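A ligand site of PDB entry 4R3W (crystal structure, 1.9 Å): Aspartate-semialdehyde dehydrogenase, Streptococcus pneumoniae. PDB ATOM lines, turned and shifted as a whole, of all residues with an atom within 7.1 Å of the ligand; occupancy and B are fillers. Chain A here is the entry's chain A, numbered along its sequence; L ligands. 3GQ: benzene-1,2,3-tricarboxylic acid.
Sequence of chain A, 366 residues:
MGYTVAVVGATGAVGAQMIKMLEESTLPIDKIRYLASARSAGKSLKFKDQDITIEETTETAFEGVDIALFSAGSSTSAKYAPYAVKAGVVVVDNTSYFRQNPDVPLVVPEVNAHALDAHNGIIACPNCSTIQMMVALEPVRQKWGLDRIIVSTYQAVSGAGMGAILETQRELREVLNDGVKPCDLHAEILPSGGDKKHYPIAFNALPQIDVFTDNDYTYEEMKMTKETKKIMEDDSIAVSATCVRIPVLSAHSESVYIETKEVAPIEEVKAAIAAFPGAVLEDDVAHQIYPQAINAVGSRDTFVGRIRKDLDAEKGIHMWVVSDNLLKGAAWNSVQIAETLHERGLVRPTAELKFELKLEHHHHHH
OAE of the ligand is in hydrogen-bond range of N of Ser 74 (2.9 Å). OG of Ser 96 is in hydrogen-bond range of OAF of the ligand. NH1 of Arg 99 is in salt-bridge range of OAD of the ligand (2.9 Å). NZ of Lys 223 lies within salt-bridge range of OAD of the ligand (2.6 Å). An oxygen (OAA) of the ligand lies within hydrogen-bond range of the side-chain amide nitrogen (ND2) of Asn 127, at 3.5 Å. The backbone NH of Ser 96 is in hydrogen-bond range of an oxygen (OAC) of the ligand. The side-chain hydroxyl (OG) of Ser 74 lies within hydrogen-bond range of an oxygen (OAC) of the ligand (3.1 Å).
CA of Gly 73 touches OAE of the ligand, at 3.4 Å. Thr 95 touches the ligand (CA to OAC, 3.2 Å). Gly 159 touches the ligand (O to CAG, 3.7 Å). Of the 28 residues printed, 8 come within 4 Å of the ligand.
The guanidinium group (NE) of Arg 99 sits at hydrogen-bond distance from the backbone carbonyl oxygen (O) of Cys 125, at 2.9 Å. The backbone carbonyl oxygen (O) of Thr 95 is in hydrogen-bond range of the guanidinium group (NE) of Arg 99, at 3.2 Å. N of Tyr 97 lies close to OG1 of Thr 95 (3.2 Å). The side-chain amino group of Lys 223 is in salt-bridge range of the side-chain carboxylate of Asp 210, 2.9 Å away. NH2 of Arg 99 is in hydrogen-bond range of O of Asn 94, 2.7 Å away. N of Tyr 97 is in hydrogen-bond range of OG of Ser 74 (3.3 Å). The side-chain hydroxyl (OG) of Ser 96 is in hydrogen-bond range of the side-chain hydroxyl (OG) of Ser 74 (2.9 Å). The side-chain carboxylate (OE1) of Glu 227 is in hydrogen-bond range of the backbone NH (N) of Asn 127, 2.9 Å away.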
ATOM      1  N   ALA A  72      26.261   8.003  29.465  1.00  0.00           N
ATOM      2  CA  ALA A  72      25.395   6.877  29.168  1.00  0.00           C
ATOM      3  C   ALA A  72      23.936   7.292  28.936  1.00  0.00           C
ATOM      4  O   ALA A  72      23.008   6.509  29.195  1.00  0.00           O
ATOM      5  CB  ALA A  72      25.492   5.870  30.307  1.00  0.00           C
ATOM      6  N   GLY A  73      23.749   8.509  28.439  1.00  0.00           N
ATOM      7  CA  GLY A  73      22.440   9.045  28.124  1.00  0.00           C
ATOM      8  C   GLY A  73      21.860   9.723  29.348  1.00  0.00           C
ATOM      9  O   GLY A  73      22.217   9.401  30.487  1.00  0.00           O
ATOM     10  N   SER A  74      20.967  10.679  29.093  1.00  0.00           N
ATOM     11  CA  SER A  74      20.360  11.509  30.122  1.00  0.00           C
ATOM     12  C   SER A  74      19.597  10.746  31.169  1.00  0.00           C
ATOM     13  O   SER A  74      19.637  11.108  32.343  1.00  0.00           O
ATOM     14  CB  SER A  74      19.388  12.523  29.493  1.00  0.00           C
ATOM     15  OG  SER A  74      20.062  13.748  29.292  1.00  0.00           O
ATOM     16  N   SER A  75      18.878   9.723  30.735  1.00  0.00           N
ATOM     17  CA  SER A  75      18.106   8.869  31.630  1.00  0.00           C
ATOM     18  C   SER A  75      18.992   8.160  32.668  1.00  0.00           C
ATOM     19  O   SER A  75      18.608   8.031  33.819  1.00  0.00           O
ATOM     20  CB  SER A  75      17.324   7.852  30.800  1.00  0.00           C
ATOM     21  OG  SER A  75      17.084   6.662  31.536  1.00  0.00           O
ATOM     22  N   THR A  76      20.173   7.718  32.252  1.00  0.00           N
ATOM     23  CA  THR A  76      21.127   7.063  33.144  1.00  0.00           C
ATOM     24  C   THR A  76      21.697   8.072  34.164  1.00  0.00           C
ATOM     25  O   THR A  76      21.824   7.752  35.346  1.00  0.00           O
ATOM     26  CB  THR A  76      22.264   6.341  32.381  1.00  0.00           C
ATOM     27  OG1 THR A  76      21.706   5.375  31.490  1.00  0.00           O
ATOM     28  CG2 THR A  76      23.204   5.614  33.305  1.00  0.00           C
ATOM     29  N   SER A  77      21.989   9.300  33.724  1.00  0.00           N
ATOM     30  CA  SER A  77      22.490  10.330  34.635  1.00  0.00           C
ATOM     31  C   SER A  77      21.401  10.725  35.649  1.00  0.00           C
ATOM     32  O   SER A  77      21.701  10.966  36.815  1.00  0.00           O
ATOM     33  CB  SER A  77      22.953  11.575  33.868  1.00  0.00           C
ATOM     34  OG  SER A  77      24.188  11.331  33.218  1.00  0.00           O
ATOM     35  N   ASP A  93      29.181  15.151  34.329  1.00  0.00           N
ATOM     36  CA  ASP A  93      28.122  14.607  33.471  1.00  0.00           C
ATOM     37  C   ASP A  93      28.161  15.150  32.033  1.00  0.00           C
ATOM     38  O   ASP A  93      28.092  16.348  31.831  1.00  0.00           O
ATOM     39  CB  ASP A  93      26.760  14.889  34.073  1.00  0.00           C
ATOM     40  CG  ASP A  93      25.647  14.133  33.360  1.00  0.00           C
ATOM     41  OD1 ASP A  93      25.942  13.130  32.678  1.00  0.00           O
ATOM     42  OD2 ASP A  93      24.473  14.556  33.459  1.00  0.00           O
ATOM     43  N   ASN A  94      28.225  14.254  31.045  1.00  0.00           N
ATOM     44  CA  ASN A  94      28.142  14.658  29.649  1.00  0.00           C
ATOM     45  C   ASN A  94      26.752  14.967  29.107  1.00  0.00           C
ATOM     46  O   ASN A  94      26.653  15.596  28.075  1.00  0.00           O
ATOM     47  CB  ASN A  94      28.769  13.611  28.730  1.00  0.00           C
ATOM     48  CG  ASN A  94      30.264  13.750  28.634  1.00  0.00           C
ATOM     49  OD1 ASN A  94      31.002  12.926  29.154  1.00  0.00           O
ATOM     50  ND2 ASN A  94      30.736  14.818  27.982  1.00  0.00           N
ATOM     51  N   THR A  95      25.705  14.557  29.813  1.00  0.00           N
ATOM     52  CA  THR A  95      24.348  14.594  29.289  1.00  0.00           C
ATOM     53  C   THR A  95      23.693  15.943  29.505  1.00  0.00           C
ATOM     54  O   THR A  95      24.229  16.795  30.217  1.00  0.00           O
ATOM     55  CB  THR A  95      23.436  13.506  29.933  1.00  0.00           C
ATOM     56  OG1 THR A  95      23.013  13.924  31.246  1.00  0.00           O
ATOM     57  CG2 THR A  95      24.140  12.151  29.995  1.00  0.00           C
ATOM     58  N   SER A  96      22.517  16.113  28.920  1.00  0.00           N
ATOM     59  CA  SER A  96      21.757  17.356  29.033  1.00  0.00           C
ATOM     60  C   SER A  96      21.010  17.490  30.351  1.00  0.00           C
ATOM     61  O   SER A  96      20.500  18.561  30.642  1.00  0.00           O
ATOM     62  CB  SER A  96      20.721  17.467  27.916  1.00  0.00           C
ATOM     63  OG  SER A  96      19.835  16.369  27.966  1.00  0.00           O
ATOM     64  N   TYR A  97      20.924  16.404  31.107  1.00  0.00           N
ATOM     65  CA  TYR A  97      19.915  16.339  32.168  1.00  0.00           C
ATOM     66  C   TYR A  97      20.062  17.422  33.233  1.00  0.00           C
ATOM     67  O   TYR A  97      19.062  18.025  33.615  1.00  0.00           O
ATOM     68  CB  TYR A  97      19.886  14.967  32.843  1.00  0.00           C
ATOM     69  CG  TYR A  97      18.649  14.826  33.675  1.00  0.00           C
ATOM     70  CD1 TYR A  97      17.429  14.524  33.081  1.00  0.00           C
ATOM     71  CD2 TYR A  97      18.697  15.025  35.051  1.00  0.00           C
ATOM     72  CE1 TYR A  97      16.282  14.405  33.854  1.00  0.00           C
ATOM     73  CE2 TYR A  97      17.544  14.911  35.830  1.00  0.00           C
ATOM     74  CZ  TYR A  97      16.349  14.616  35.223  1.00  0.00           C
ATOM     75  OH  TYR A  97      15.221  14.504  35.975  1.00  0.00           O
ATOM     76  N   ARG A  99      22.147  20.241  32.939  1.00  0.00           N
ATOM     77  CA  ARG A  99      22.855  21.416  32.426  1.00  0.00           C
ATOM     78  C   ARG A  99      22.231  22.756  32.820  1.00  0.00           C
ATOM     79  O   ARG A  99      22.966  23.727  32.992  1.00  0.00           O
ATOM     80  CB  ARG A  99      22.977  21.371  30.908  1.00  0.00           C
ATOM     81  CG  ARG A  99      23.864  20.255  30.362  1.00  0.00           C
ATOM     82  CD  ARG A  99      23.930  20.355  28.861  1.00  0.00           C
ATOM     83  NE  ARG A  99      24.786  19.310  28.320  1.00  0.00           N
ATOM     84  CZ  ARG A  99      24.548  18.624  27.218  1.00  0.00           C
ATOM     85  NH1 ARG A  99      23.489  18.887  26.456  1.00  0.00           N
ATOM     86  NH2 ARG A  99      25.410  17.691  26.843  1.00  0.00           N
ATOM     87  N   CYS A 125      29.043  18.958  31.430  1.00  0.00           N
ATOM     88  CA  CYS A 125      29.683  19.239  30.162  1.00  0.00           C
ATOM     89  C   CYS A 125      28.575  19.671  29.182  1.00  0.00           C
ATOM     90  O   CYS A 125      27.558  18.965  29.074  1.00  0.00           O
ATOM     91  CB  CYS A 125      30.357  17.950  29.674  1.00  0.00           C
ATOM     92  SG  CYS A 125      31.387  18.032  28.197  1.00  0.00           S
ATOM     93  N   PRO A 126      28.739  20.837  28.490  1.00  0.00           N
ATOM     94  CA  PRO A 126      27.717  21.239  27.526  1.00  0.00           C
ATOM     95  C   PRO A 126      27.668  20.295  26.340  1.00  0.00           C
ATOM     96  O   PRO A 126      28.521  19.426  26.188  1.00  0.00           O
ATOM     97  CB  PRO A 126      28.150  22.651  27.074  1.00  0.00           C
ATOM     98  CG  PRO A 126      29.242  23.066  27.996  1.00  0.00           C
ATOM     99  CD  PRO A 126      29.850  21.787  28.537  1.00  0.00           C
ATOM    100  N   ASN A 127      26.631  20.441  25.549  1.00  0.00           N
ATOM    101  CA  ASN A 127      26.509  19.790  24.252  1.00  0.00           C
ATOM    102  C   ASN A 127      27.726  20.028  23.348  1.00  0.00           C
ATOM    103  O   ASN A 127      28.288  21.132  23.339  1.00  0.00           O
ATOM    104  CB  ASN A 127      25.246  20.341  23.599  1.00  0.00           C
ATOM    105  CG  ASN A 127      25.122  19.914  22.170  1.00  0.00           C
ATOM    106  OD1 ASN A 127      25.404  20.697  21.273  1.00  0.00           O
ATOM    107  ND2 ASN A 127      24.766  18.658  21.952  1.00  0.00           N
ATOM    108  N   CYS A 128      28.114  19.016  22.551  1.00  0.00           N
ATOM    109  CA  CYS A 128      29.311  19.089  21.702  1.00  0.00           C
ATOM    110  C   CYS A 128      29.367  20.321  20.785  1.00  0.00           C
ATOM    111  O   CYS A 128      30.411  20.969  20.650  1.00  0.00           O
ATOM    112  CB  CYS A 128      29.445  17.799  20.877  1.00  0.00           C
ATOM    113  SG  CYS A 128      27.911  17.093  20.184  1.00  0.00           S
ATOM    114  N   GLY A 159      27.969  11.594  17.374  1.00  0.00           N
ATOM    115  CA  GLY A 159      27.209  12.226  18.430  1.00  0.00           C
ATOM    116  C   GLY A 159      25.940  11.488  18.814  1.00  0.00           C
ATOM    117  O   GLY A 159      25.489  11.637  19.940  1.00  0.00           O
ATOM    118  N   ALA A 160      25.344  10.719  17.896  1.00  0.00           N
ATOM    119  CA  ALA A 160      24.134   9.972  18.232  1.00  0.00           C
ATOM    120  C   ALA A 160      24.433   8.550  18.721  1.00  0.00           C
ATOM    121  O   ALA A 160      23.506   7.786  18.930  1.00  0.00           O
ATOM    122  CB  ALA A 160      23.167   9.923  17.056  1.00  0.00           C
ATOM    123  N   GLY A 161      25.717   8.200  18.863  1.00  0.00           N
ATOM    124  CA  GLY A 161      26.130   6.923  19.468  1.00  0.00           C
ATOM    125  C   GLY A 161      26.656   5.868  18.498  1.00  0.00           C
ATOM    126  O   GLY A 161      26.626   6.028  17.270  1.00  0.00           O
ATOM    127  N   GLY A 194      15.062   8.568  19.856  1.00  0.00           N
ATOM    128  CA  GLY A 194      13.827   8.856  20.587  1.00  0.00           C
ATOM    129  C   GLY A 194      12.582   9.229  19.769  1.00  0.00           C
ATOM    130  O   GLY A 194      11.506   9.340  20.330  1.00  0.00           O
ATOM    131  N   ILE A 209      18.035  17.296  14.690  1.00  0.00           N
ATOM    132  CA  ILE A 209      18.914  16.707  15.682  1.00  0.00           C
ATOM    133  C   ILE A 209      18.145  16.812  17.001  1.00  0.00           C
ATOM    134  O   ILE A 209      17.670  17.889  17.342  1.00  0.00           O
ATOM    135  CB  ILE A 209      20.273  17.447  15.768  1.00  0.00           C
ATOM    136  CG1 ILE A 209      21.017  17.248  14.435  1.00  0.00           C
ATOM    137  CG2 ILE A 209      21.111  16.905  16.932  1.00  0.00           C
ATOM    138  CD1 ILE A 209      22.372  17.885  14.351  1.00  0.00           C
ATOM    139  N   ASP A 210      18.001  15.694  17.707  1.00  0.00           N
ATOM    140  CA  ASP A 210      17.086  15.587  18.853  1.00  0.00           C
ATOM    141  C   ASP A 210      15.633  15.744  18.410  1.00  0.00           C
ATOM    142  O   ASP A 210      15.346  15.832  17.226  1.00  0.00           O
ATOM    143  CB  ASP A 210      17.428  16.610  19.941  1.00  0.00           C
ATOM    144  CG  ASP A 210      17.187  16.082  21.356  1.00  0.00           C
ATOM    145  OD1 ASP A 210      16.186  15.347  21.596  1.00  0.00           O
ATOM    146  OD2 ASP A 210      18.003  16.420  22.237  1.00  0.00           O
ATOM    147  N   TYR A 219      15.351  20.443  20.199  1.00  0.00           N
ATOM    148  CA  TYR A 219      16.043  20.477  21.470  1.00  0.00           C
ATOM    149  C   TYR A 219      17.517  20.764  21.308  1.00  0.00           C
ATOM    150  O   TYR A 219      18.091  21.385  22.159  1.00  0.00           O
ATOM    151  CB  TYR A 219      15.860  19.185  22.268  1.00  0.00           C
ATOM    152  CG  TYR A 219      14.634  19.203  23.161  1.00  0.00           C
ATOM    153  CD1 TYR A 219      14.693  19.660  24.476  1.00  0.00           C
ATOM    154  CD2 TYR A 219      13.403  18.778  22.663  1.00  0.00           C
ATOM    155  CE1 TYR A 219      13.538  19.676  25.276  1.00  0.00           C
ATOM    156  CE2 TYR A 219      12.264  18.786  23.434  1.00  0.00           C
ATOM    157  CZ  TYR A 219      12.327  19.231  24.731  1.00  0.00           C
ATOM    158  OH  TYR A 219      11.157  19.223  25.433  1.00  0.00           O
ATOM    159  N   GLU A 220      18.126  20.292  20.222  1.00  0.00           N
ATOM    160  CA  GLU A 220      19.533  20.561  19.988  1.00  0.00           C
ATOM    161  C   GLU A 220      19.734  22.052  19.699  1.00  0.00           C
ATOM    162  O   GLU A 220      20.684  22.658  20.216  1.00  0.00           O
ATOM    163  CB  GLU A 220      20.067  19.710  18.833  1.00  0.00           C
ATOM    164  CG  GLU A 220      21.505  20.002  18.440  1.00  0.00           C
ATOM    165  CD  GLU A 220      22.538  19.406  19.400  1.00  0.00           C
ATOM    166  OE1 GLU A 220      22.125  18.895  20.462  1.00  0.00           O
ATOM    167  OE2 GLU A 220      23.758  19.435  19.073  1.00  0.00           O
ATOM    168  N   LYS A 223      19.167  23.830  23.076  1.00  0.00           N
ATOM    169  CA  LYS A 223      20.352  23.616  23.913  1.00  0.00           C
ATOM    170  C   LYS A 223      21.464  24.589  23.566  1.00  0.00           C
ATOM    171  O   LYS A 223      22.067  25.141  24.459  1.00  0.00           O
ATOM    172  CB  LYS A 223      20.887  22.192  23.770  1.00  0.00           C
ATOM    173  CG  LYS A 223      20.072  21.152  24.493  1.00  0.00           C
ATOM    174  CD  LYS A 223      20.526  19.753  24.089  1.00  0.00           C
ATOM    175  CE  LYS A 223      19.552  18.700  24.585  1.00  0.00           C
ATOM    176  NZ  LYS A 223      19.976  17.329  24.193  1.00  0.00           N
ATOM    177  N   GLU A 227      22.412  27.010  26.546  1.00  0.00           N
ATOM    178  CA  GLU A 227      23.728  26.704  27.093  1.00  0.00           C
ATOM    179  C   GLU A 227      24.670  27.861  26.881  1.00  0.00           C
ATOM    180  O   GLU A 227      25.427  28.204  27.780  1.00  0.00           O
ATOM    181  CB  GLU A 227      24.292  25.419  26.485  1.00  0.00           C
ATOM    182  CG  GLU A 227      23.515  24.200  26.963  1.00  0.00           C
ATOM    183  CD  GLU A 227      23.910  22.923  26.269  1.00  0.00           C
ATOM    184  OE1 GLU A 227      24.996  22.886  25.653  1.00  0.00           O
ATOM    185  OE2 GLU A 227      23.130  21.946  26.343  1.00  0.00           O
ATOM    186  N   ARG A 245      22.298  17.147  10.607  1.00  0.00           N
ATOM    187  CA  ARG A 245      23.155  15.965  10.511  1.00  0.00           C
ATOM    188  C   ARG A 245      23.599  15.697   9.072  1.00  0.00           C
ATOM    189  O   ARG A 245      22.780  15.707   8.156  1.00  0.00           O
ATOM    190  CB  ARG A 245      22.421  14.747  11.016  1.00  0.00           C
ATOM    191  CG  ARG A 245      23.314  13.567  11.314  1.00  0.00           C
ATOM    192  CD  ARG A 245      23.994  13.678  12.658  1.00  0.00           C
ATOM    193  NE  ARG A 245      23.044  13.566  13.753  1.00  0.00           N
ATOM    194  CZ  ARG A 245      23.325  13.739  15.044  1.00  0.00           C
ATOM    195  NH1 ARG A 245      24.556  14.012  15.436  1.00  0.00           N
ATOM    196  NH2 ARG A 245      22.359  13.633  15.946  1.00  0.00           N
ATOM    197  N   GLY A 329      34.312  18.076  22.145  1.00  0.00           N
ATOM    198  CA  GLY A 329      32.878  17.991  22.223  1.00  0.00           C
ATOM    199  C   GLY A 329      32.353  17.122  23.344  1.00  0.00           C
ATOM    200  O   GLY A 329      31.198  17.247  23.690  1.00  0.00           O
HETATM  201  OAC 3GQ L   1      22.121  14.164  27.069  1.00  0.00           O
HETATM  202  CAL 3GQ L   1      21.414  14.183  26.060  1.00  0.00           C
HETATM  203  OAF 3GQ L   1      20.249  14.633  26.128  1.00  0.00           O
HETATM  204  CAO 3GQ L   1      21.951  13.697  24.861  1.00  0.00           C
HETATM  205  CAM 3GQ L   1      22.835  14.513  24.135  1.00  0.00           C
HETATM  206  CAJ 3GQ L   1      23.202  15.819  24.540  1.00  0.00           C
HETATM  207  OAD 3GQ L   1      22.366  16.629  24.985  1.00  0.00           O
HETATM  208  OAA 3GQ L   1      24.378  16.226  24.383  1.00  0.00           O
HETATM  209  CAH 3GQ L   1      23.362  14.016  22.934  1.00  0.00           C
HETATM  210  CAG 3GQ L   1      23.038  12.742  22.460  1.00  0.00           C
HETATM  211  CAI 3GQ L   1      22.172  11.937  23.194  1.00  0.00           C
HETATM  212  CAN 3GQ L   1      21.623  12.411  24.409  1.00  0.00           C
HETATM  213  CAK 3GQ L   1      20.742  11.542  25.082  1.00  0.00           C
HETATM  214  OAE 3GQ L   1      20.725  11.434  26.334  1.00  0.00           O
HETATM  215  OAB 3GQ L   1      19.942  10.860  24.401  1.00  0.00           O
